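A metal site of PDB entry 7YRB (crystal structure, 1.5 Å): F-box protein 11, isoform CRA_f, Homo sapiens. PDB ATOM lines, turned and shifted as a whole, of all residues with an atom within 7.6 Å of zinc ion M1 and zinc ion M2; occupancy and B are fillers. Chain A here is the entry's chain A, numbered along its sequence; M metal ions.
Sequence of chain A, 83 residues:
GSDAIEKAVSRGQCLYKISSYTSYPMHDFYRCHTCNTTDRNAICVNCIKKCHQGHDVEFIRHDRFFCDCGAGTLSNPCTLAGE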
ATOM      1  N   GLN A  13       0.664  10.238   8.441  1.00  0.00           N
ATOM      2  CA  GLN A  13       1.828  10.871   9.033  1.00  0.00           C
ATOM      3  C   GLN A  13       2.803   9.791   9.513  1.00  0.00           C
ATOM      4  O   GLN A  13       2.475   8.606   9.640  1.00  0.00           O
ATOM      5  CB  GLN A  13       1.388  11.809  10.167  1.00  0.00           C
ATOM      6  CG  GLN A  13       0.646  13.152   9.801  1.00  0.00           C
ATOM      7  CD  GLN A  13       1.153  13.941   8.564  1.00  0.00           C
ATOM      8  OE1 GLN A  13       2.309  14.366   8.491  1.00  0.00           O
ATOM      9  NE2 GLN A  13       0.231  14.195   7.615  1.00  0.00           N
ATOM     10  N   CYS A  14       4.031  10.218   9.789  1.00  0.00           N
ATOM     11  CA  CYS A  14       5.008   9.323  10.376  1.00  0.00           C
ATOM     12  C   CYS A  14       4.785   9.155  11.873  1.00  0.00           C
ATOM     13  O   CYS A  14       4.550  10.135  12.601  1.00  0.00           O
ATOM     14  CB  CYS A  14       6.426   9.842  10.157  1.00  0.00           C
ATOM     15  SG  CYS A  14       7.770   8.890  11.017  1.00  0.00           S
ATOM     16  N   LEU A  15       4.857   7.925  12.343  1.00  0.00           N
ATOM     17  CA  LEU A  15       4.573   7.670  13.749  1.00  0.00           C
ATOM     18  C   LEU A  15       5.612   8.260  14.697  1.00  0.00           C
ATOM     19  O   LEU A  15       5.357   8.343  15.905  1.00  0.00           O
ATOM     20  CB  LEU A  15       4.452   6.181  13.978  1.00  0.00           C
ATOM     21  CG  LEU A  15       3.196   5.529  13.406  1.00  0.00           C
ATOM     22  CD1 LEU A  15       3.169   4.058  13.668  1.00  0.00           C
ATOM     23  CD2 LEU A  15       1.914   6.169  13.966  1.00  0.00           C
ATOM     24  N   TYR A  16       6.775   8.669  14.208  1.00  0.00           N
ATOM     25  CA  TYR A  16       7.738   9.303  15.094  1.00  0.00           C
ATOM     26  C   TYR A  16       7.196  10.597  15.676  1.00  0.00           C
ATOM     27  O   TYR A  16       7.633  11.018  16.758  1.00  0.00           O
ATOM     28  CB  TYR A  16       9.030   9.539  14.325  1.00  0.00           C
ATOM     29  CG  TYR A  16      10.172   9.979  15.185  1.00  0.00           C
ATOM     30  CD1 TYR A  16      10.895   9.053  15.921  1.00  0.00           C
ATOM     31  CD2 TYR A  16      10.537  11.301  15.244  1.00  0.00           C
ATOM     32  CE1 TYR A  16      11.941   9.452  16.695  1.00  0.00           C
ATOM     33  CE2 TYR A  16      11.595  11.708  16.022  1.00  0.00           C
ATOM     34  CZ  TYR A  16      12.296  10.775  16.755  1.00  0.00           C
ATOM     35  OH  TYR A  16      13.362  11.168  17.538  1.00  0.00           O
ATOM     36  N   LYS A  17       6.261  11.245  14.992  1.00  0.00           N
ATOM     37  CA  LYS A  17       5.705  12.512  15.455  1.00  0.00           C
ATOM     38  C   LYS A  17       4.877  12.348  16.714  1.00  0.00           C
ATOM     39  O   LYS A  17       4.524  13.358  17.352  1.00  0.00           O
ATOM     40  CB  LYS A  17       4.826  13.148  14.380  1.00  0.00           C
ATOM     41  CG  LYS A  17       5.566  13.589  13.132  1.00  0.00           C
ATOM     42  CD  LYS A  17       6.580  14.690  13.388  1.00  0.00           C
ATOM     43  CE  LYS A  17       7.182  15.080  12.038  1.00  0.00           C
ATOM     44  NZ  LYS A  17       7.999  16.314  12.049  1.00  0.00           N
ATOM     45  N   ALA A  42      13.740  -0.115  11.686  1.00  0.00           N
ATOM     46  CA  ALA A  42      12.289  -0.303  11.767  1.00  0.00           C
ATOM     47  C   ALA A  42      11.627   0.960  11.254  1.00  0.00           C
ATOM     48  O   ALA A  42      11.937   2.059  11.718  1.00  0.00           O
ATOM     49  CB  ALA A  42      11.833  -0.568  13.195  1.00  0.00           C
ATOM     50  N   ILE A  43      10.769   0.809  10.242  1.00  0.00           N
ATOM     51  CA  ILE A  43      10.170   1.930   9.524  1.00  0.00           C
ATOM     52  C   ILE A  43       8.653   1.787   9.512  1.00  0.00           C
ATOM     53  O   ILE A  43       8.123   0.694   9.257  1.00  0.00           O
ATOM     54  CB  ILE A  43      10.727   2.024   8.086  1.00  0.00           C
ATOM     55  CG1 ILE A  43      12.263   2.159   8.138  1.00  0.00           C
ATOM     56  CG2 ILE A  43      10.098   3.156   7.296  1.00  0.00           C
ATOM     57  CD1 ILE A  43      12.937   2.136   6.766  1.00  0.00           C
ATOM     58  N   CYS A  44       7.947   2.895   9.744  1.00  0.00           N
ATOM     59  CA  CYS A  44       6.493   2.859   9.799  1.00  0.00           C
ATOM     60  C   CYS A  44       5.907   2.730   8.386  1.00  0.00           C
ATOM     61  O   CYS A  44       6.588   2.917   7.379  1.00  0.00           O
ATOM     62  CB  CYS A  44       5.967   4.111  10.505  1.00  0.00           C
ATOM     63  SG  CYS A  44       5.940   5.660   9.583  1.00  0.00           S
ATOM     64  N   VAL A  45       4.615   2.354   8.323  1.00  0.00           N
ATOM     65  CA  VAL A  45       4.046   2.015   7.021  1.00  0.00           C
ATOM     66  C   VAL A  45       3.960   3.233   6.104  1.00  0.00           C
ATOM     67  O   VAL A  45       4.152   3.116   4.890  1.00  0.00           O
ATOM     68  CB  VAL A  45       2.662   1.356   7.175  1.00  0.00           C
ATOM     69  CG1 VAL A  45       1.670   2.331   7.761  1.00  0.00           C
ATOM     70  CG2 VAL A  45       2.185   0.776   5.823  1.00  0.00           C
ATOM     71  N   ASN A  46       3.699   4.428   6.658  1.00  0.00           N
ATOM     72  CA  ASN A  46       3.597   5.591   5.773  1.00  0.00           C
ATOM     73  C   ASN A  46       4.956   5.968   5.225  1.00  0.00           C
ATOM     74  O   ASN A  46       5.046   6.359   4.048  1.00  0.00           O
ATOM     75  CB  ASN A  46       2.950   6.756   6.514  1.00  0.00           C
ATOM     76  CG  ASN A  46       1.464   6.520   6.725  1.00  0.00           C
ATOM     77  OD1 ASN A  46       0.800   5.955   5.847  1.00  0.00           O
ATOM     78  ND2 ASN A  46       0.950   6.900   7.891  1.00  0.00           N
ATOM     79  N   CYS A  47       6.013   5.845   6.027  1.00  0.00           N
ATOM     80  CA  CYS A  47       7.357   6.087   5.522  1.00  0.00           C
ATOM     81  C   CYS A  47       7.766   5.053   4.499  1.00  0.00           C
ATOM     82  O   CYS A  47       8.375   5.400   3.466  1.00  0.00           O
ATOM     83  CB  CYS A  47       8.341   6.096   6.687  1.00  0.00           C
ATOM     84  SG  CYS A  47       8.310   7.617   7.629  1.00  0.00           S
ATOM     85  N   ILE A  48       7.429   3.781   4.709  1.00  0.00           N
ATOM     86  CA  ILE A  48       7.891   2.773   3.742  1.00  0.00           C
ATOM     87  C   ILE A  48       7.256   2.997   2.382  1.00  0.00           C
ATOM     88  O   ILE A  48       7.871   2.702   1.352  1.00  0.00           O
ATOM     89  CB  ILE A  48       7.649   1.345   4.281  1.00  0.00           C
ATOM     90  CG1 ILE A  48       8.744   0.392   3.772  1.00  0.00           C
ATOM     91  CG2 ILE A  48       6.251   0.849   3.928  1.00  0.00           C
ATOM     92  CD1 ILE A  48      10.131   0.698   4.329  1.00  0.00           C
ATOM     93  N   LYS A  50       6.186   5.993   1.167  1.00  0.00           N
ATOM     94  CA  LYS A  50       6.504   7.290   0.578  1.00  0.00           C
ATOM     95  C   LYS A  50       8.005   7.560   0.576  1.00  0.00           C
ATOM     96  O   LYS A  50       8.618   7.682  -0.493  1.00  0.00           O
ATOM     97  CB  LYS A  50       5.740   8.397   1.336  1.00  0.00           C
ATOM     98  CG  LYS A  50       5.925   9.768   0.739  1.00  0.00           C
ATOM     99  CD  LYS A  50       4.808  10.713   1.115  1.00  0.00           C
ATOM    100  CE  LYS A  50       4.898  11.964   0.250  1.00  0.00           C
ATOM    101  NZ  LYS A  50       5.998  12.838   0.721  1.00  0.00           N
ATOM    102  N   CYS A  51       8.637   7.577   1.741  1.00  0.00           N
ATOM    103  CA  CYS A  51      10.065   7.824   1.844  1.00  0.00           C
ATOM    104  C   CYS A  51      10.891   6.724   1.211  1.00  0.00           C
ATOM    105  O   CYS A  51      12.065   6.961   0.848  1.00  0.00           O
ATOM    106  CB  CYS A  51      10.461   7.961   3.317  1.00  0.00           C
ATOM    107  SG  CYS A  51       9.379   9.096   4.233  1.00  0.00           S
ATOM    108  N   HIS A  52      10.349   5.516   1.082  1.00  0.00           N
ATOM    109  CA  HIS A  52      11.102   4.396   0.546  1.00  0.00           C
ATOM    110  C   HIS A  52      10.410   3.769  -0.650  1.00  0.00           C
ATOM    111  O   HIS A  52      10.615   2.596  -0.950  1.00  0.00           O
ATOM    112  CB  HIS A  52      11.393   3.377   1.637  1.00  0.00           C
ATOM    113  CG  HIS A  52      12.087   4.014   2.783  1.00  0.00           C
ATOM    114  ND1 HIS A  52      13.449   4.131   2.875  1.00  0.00           N
ATOM    115  CD2 HIS A  52      11.577   4.610   3.896  1.00  0.00           C
ATOM    116  CE1 HIS A  52      13.759   4.756   4.001  1.00  0.00           C
ATOM    117  NE2 HIS A  52      12.633   5.085   4.615  1.00  0.00           N
ATOM    118  N   PHE A  65       7.769  -0.415  18.199  1.00  0.00           N
ATOM    119  CA  PHE A  65       8.932   0.180  17.547  1.00  0.00           C
ATOM    120  C   PHE A  65       8.784   1.688  17.617  1.00  0.00           C
ATOM    121  O   PHE A  65       7.687   2.203  17.843  1.00  0.00           O
ATOM    122  CB  PHE A  65       9.068  -0.320  16.091  1.00  0.00           C
ATOM    123  CG  PHE A  65       8.109   0.307  15.117  1.00  0.00           C
ATOM    124  CD1 PHE A  65       6.778  -0.059  15.121  1.00  0.00           C
ATOM    125  CD2 PHE A  65       8.531   1.221  14.185  1.00  0.00           C
ATOM    126  CE1 PHE A  65       5.882   0.504  14.232  1.00  0.00           C
ATOM    127  CE2 PHE A  65       7.635   1.782  13.274  1.00  0.00           C
ATOM    128  CZ  PHE A  65       6.325   1.416  13.300  1.00  0.00           C
ATOM    129  N   PHE A  66       9.871   2.395  17.298  1.00  0.00           N
ATOM    130  CA  PHE A  66       9.776   3.770  16.853  1.00  0.00           C
ATOM    131  C   PHE A  66      10.466   3.879  15.502  1.00  0.00           C
ATOM    132  O   PHE A  66      11.437   3.146  15.205  1.00  0.00           O
ATOM    133  CB  PHE A  66      10.331   4.784  17.886  1.00  0.00           C
ATOM    134  CG  PHE A  66      11.832   4.782  18.044  1.00  0.00           C
ATOM    135  CD1 PHE A  66      12.651   5.380  17.109  1.00  0.00           C
ATOM    136  CD2 PHE A  66      12.425   4.205  19.163  1.00  0.00           C
ATOM    137  CE1 PHE A  66      14.023   5.397  17.259  1.00  0.00           C
ATOM    138  CE2 PHE A  66      13.797   4.222  19.312  1.00  0.00           C
ATOM    139  CZ  PHE A  66      14.596   4.816  18.365  1.00  0.00           C
ATOM    140  N   CYS A  67       9.940   4.769  14.662  1.00  0.00           N
ATOM    141  CA  CYS A  67      10.299   4.802  13.245  1.00  0.00           C
ATOM    142  C   CYS A  67      11.680   5.436  13.049  1.00  0.00           C
ATOM    143  O   CYS A  67      11.869   6.624  13.328  1.00  0.00           O
ATOM    144  CB  CYS A  67       9.257   5.579  12.436  1.00  0.00           C
ATOM    145  SG  CYS A  67       9.676   5.618  10.690  1.00  0.00           S
ATOM    146  N   ASP A  68      12.643   4.643  12.556  1.00  0.00           N
ATOM    147  CA  ASP A  68      13.990   5.159  12.311  1.00  0.00           C
ATOM    148  C   ASP A  68      14.048   6.152  11.159  1.00  0.00           C
ATOM    149  O   ASP A  68      14.987   6.959  11.089  1.00  0.00           O
ATOM    150  CB  ASP A  68      14.940   3.988  12.032  1.00  0.00           C
ATOM    151  CG  ASP A  68      15.181   3.143  13.245  1.00  0.00           C
ATOM    152  OD1 ASP A  68      15.233   3.719  14.351  1.00  0.00           O
ATOM    153  OD2 ASP A  68      15.300   1.912  13.113  1.00  0.00           O
ATOM    154  N   CYS A  69      13.110   6.092  10.212  1.00  0.00           N
ATOM    155  CA  CYS A  69      13.059   7.095   9.146  1.00  0.00           C
ATOM    156  C   CYS A  69      12.767   8.462   9.714  1.00  0.00           C
ATOM    157  O   CYS A  69      13.521   9.420   9.514  1.00  0.00           O
ATOM    158  CB  CYS A  69      12.021   6.690   8.089  1.00  0.00           C
ATOM    159  SG  CYS A  69      12.024   7.661   6.603  1.00  0.00           S
ATOM    160  N   GLY A  70      11.687   8.577  10.492  1.00  0.00           N
ATOM    161  CA  GLY A  70      11.344   9.846  11.104  1.00  0.00           C
ATOM    162  C   GLY A  70      12.359  10.313  12.120  1.00  0.00           C
ATOM    163  O   GLY A  70      12.530  11.521  12.331  1.00  0.00           O
ATOM    164  N   ALA A  71      13.039   9.371  12.773  1.00  0.00           N
ATOM    165  CA  ALA A  71      14.064   9.748  13.743  1.00  0.00           C
ATOM    166  C   ALA A  71      15.280  10.366  13.070  1.00  0.00           C
ATOM    167  O   ALA A  71      16.128  10.969  13.745  1.00  0.00           O
ATOM    168  CB  ALA A  71      14.459   8.513  14.558  1.00  0.00           C
ATOM    169  N   LEU A  74      18.462   7.247   9.051  1.00  0.00           N
ATOM    170  CA  LEU A  74      18.713   6.512   7.818  1.00  0.00           C
ATOM    171  C   LEU A  74      19.479   7.353   6.807  1.00  0.00           C
ATOM    172  O   LEU A  74      19.601   8.572   6.923  1.00  0.00           O
ATOM    173  CB  LEU A  74      17.415   6.022   7.181  1.00  0.00           C
ATOM    174  CG  LEU A  74      16.492   5.142   8.041  1.00  0.00           C
ATOM    175  CD1 LEU A  74      15.284   4.739   7.215  1.00  0.00           C
ATOM    176  CD2 LEU A  74      17.220   3.925   8.554  1.00  0.00           C
ATOM    177  N   ASN A  76      18.755   8.523   4.130  1.00  0.00           N
ATOM    178  CA  ASN A  76      17.989   9.503   3.381  1.00  0.00           C
ATOM    179  C   ASN A  76      17.044  10.257   4.313  1.00  0.00           C
ATOM    180  O   ASN A  76      16.624   9.720   5.331  1.00  0.00           O
ATOM    181  CB  ASN A  76      17.206   8.794   2.278  1.00  0.00           C
ATOM    182  CG  ASN A  76      17.904   8.879   0.929  1.00  0.00           C
ATOM    183  OD1 ASN A  76      18.494   9.909   0.600  1.00  0.00           O
ATOM    184  ND2 ASN A  76      17.874   7.782   0.164  1.00  0.00           N
ATOM    185  N   PRO A  77      16.724  11.515   4.006  1.00  0.00           N
ATOM    186  CA  PRO A  77      15.850  12.272   4.909  1.00  0.00           C
ATOM    187  C   PRO A  77      14.383  11.870   4.774  1.00  0.00           C
ATOM    188  O   PRO A  77      13.917  11.457   3.706  1.00  0.00           O
ATOM    189  CB  PRO A  77      16.076  13.727   4.467  1.00  0.00           C
ATOM    190  CG  PRO A  77      16.378  13.614   3.000  1.00  0.00           C
ATOM    191  CD  PRO A  77      17.152  12.310   2.832  1.00  0.00           C
ATOM    192  N   CYS A  78      13.667  11.984   5.879  1.00  0.00           N
ATOM    193  CA  CYS A  78      12.248  11.637   5.887  1.00  0.00           C
ATOM    194  C   CYS A  78      11.449  12.687   5.110  1.00  0.00           C
ATOM    195  O   CYS A  78      11.559  13.883   5.367  1.00  0.00           O
ATOM    196  CB  CYS A  78      11.731  11.539   7.325  1.00  0.00           C
ATOM    197  SG  CYS A  78      10.024  10.958   7.485  1.00  0.00           S
ATOM    198  N   THR A  79      10.626  12.227   4.181  1.00  0.00           N
ATOM    199  CA  THR A  79       9.770  13.126   3.417  1.00  0.00           C
ATOM    200  C   THR A  79       8.461  13.441   4.115  1.00  0.00           C
ATOM    201  O   THR A  79       7.636  14.168   3.553  1.00  0.00           O
ATOM    202  CB  THR A  79       9.454  12.544   2.050  1.00  0.00           C
ATOM    203  OG1 THR A  79       8.469  11.505   2.196  1.00  0.00           O
ATOM    204  CG2 THR A  79      10.706  11.996   1.407  1.00  0.00           C
ATOM    205  N   LEU A  80       8.220  12.870   5.299  1.00  0.00           N
ATOM    206  CA  LEU A  80       7.031  13.170   6.082  1.00  0.00           C
ATOM    207  C   LEU A  80       7.321  14.061   7.281  1.00  0.00           C
ATOM    208  O   LEU A  80       6.443  14.262   8.112  1.00  0.00           O
ATOM    209  CB  LEU A  80       6.389  11.860   6.555  1.00  0.00           C
ATOM    210  CG  LEU A  80       5.715  11.049   5.458  1.00  0.00           C
ATOM    211  CD1 LEU A  80       5.398   9.669   5.981  1.00  0.00           C
ATOM    212  CD2 LEU A  80       4.420  11.704   4.967  1.00  0.00           C
ATOM    213  N   ALA A  81       8.539  14.577   7.397  1.00  0.00           N
ATOM    214  CA  ALA A  81       8.944  15.327   8.587  1.00  0.00           C
ATOM    215  C   ALA A  81       9.183  16.803   8.304  1.00  0.00           C
ATOM    216  O   ALA A  81       9.741  17.496   9.165  1.00  0.00           O
ATOM    217  CB  ALA A  81      10.182  14.689   9.213  1.00  0.00           C
HETATM  218 ZN    ZN M   1      10.000   8.875   6.553  1.00  0.00          ZN
HETATM  219 ZN    ZN M   2       7.917   6.904   9.850  1.00  0.00          ZN
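The side-chain sulfur (SG) of Cys 14 sits close to the backbone NH (N) of Tyr 16 (3.3 Å).
The backbone carbonyl oxygen (O) of Cys 47 sits at hydrogen-bond distance from the backbone NH (N) of His 52 (3.1 Å).
SG of Cys 67 sits close to N of Cys 69 (3.5 Å).
N of Leu 80 sits close to SG of Cys 78, 3.4 Å away.
The side-chain sulfur (SG) of Cys 69 lies close to a ring nitrogen (NE2) of His 52, at 3.3 Å.
The side-chain sulfur of Cys 44 lies close to the backbone NH of Leu 15 (3.7 Å).
The backbone NH of Gly 70 lies close to the side-chain sulfur of Cys 67, at 3.6 Å.
The side-chain sulfur (SG) of Cys 51 sits close to the side-chain hydroxyl (OG1) of Thr 79 (3.3 Å).
Four residues have an atom within 4 Å of zinc ion M1: Cys 47, Cys 51, Cys 69 and Cys 78.
The nearest printed residue that does not touch zinc ion M1 is Thr 79 (4.2 Å).
The side-chain sulfur (SG) of Cys 78 binds zinc ion M1, at 2.3 Å.
SG of Cys 69 binds zinc ion M1 (2.4 Å).
SG of Cys 47 is bound to zinc ion M1, at 2.4 Å.
SG of Cys 51 is bound to zinc ion M1 (2.4 Å).
Zinc ion M1 has four donor atoms within binding distance.
SG of Cys 14 is bound to zinc ion M2, at 2.3 Å.
SG of Cys 67 binds zinc ion M2, at 2.3 Å.
SG of Cys 44 is bound to zinc ion M2 (2.4 Å).
SG of Cys 47 is bound to zinc ion M2, at 2.4 Å.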
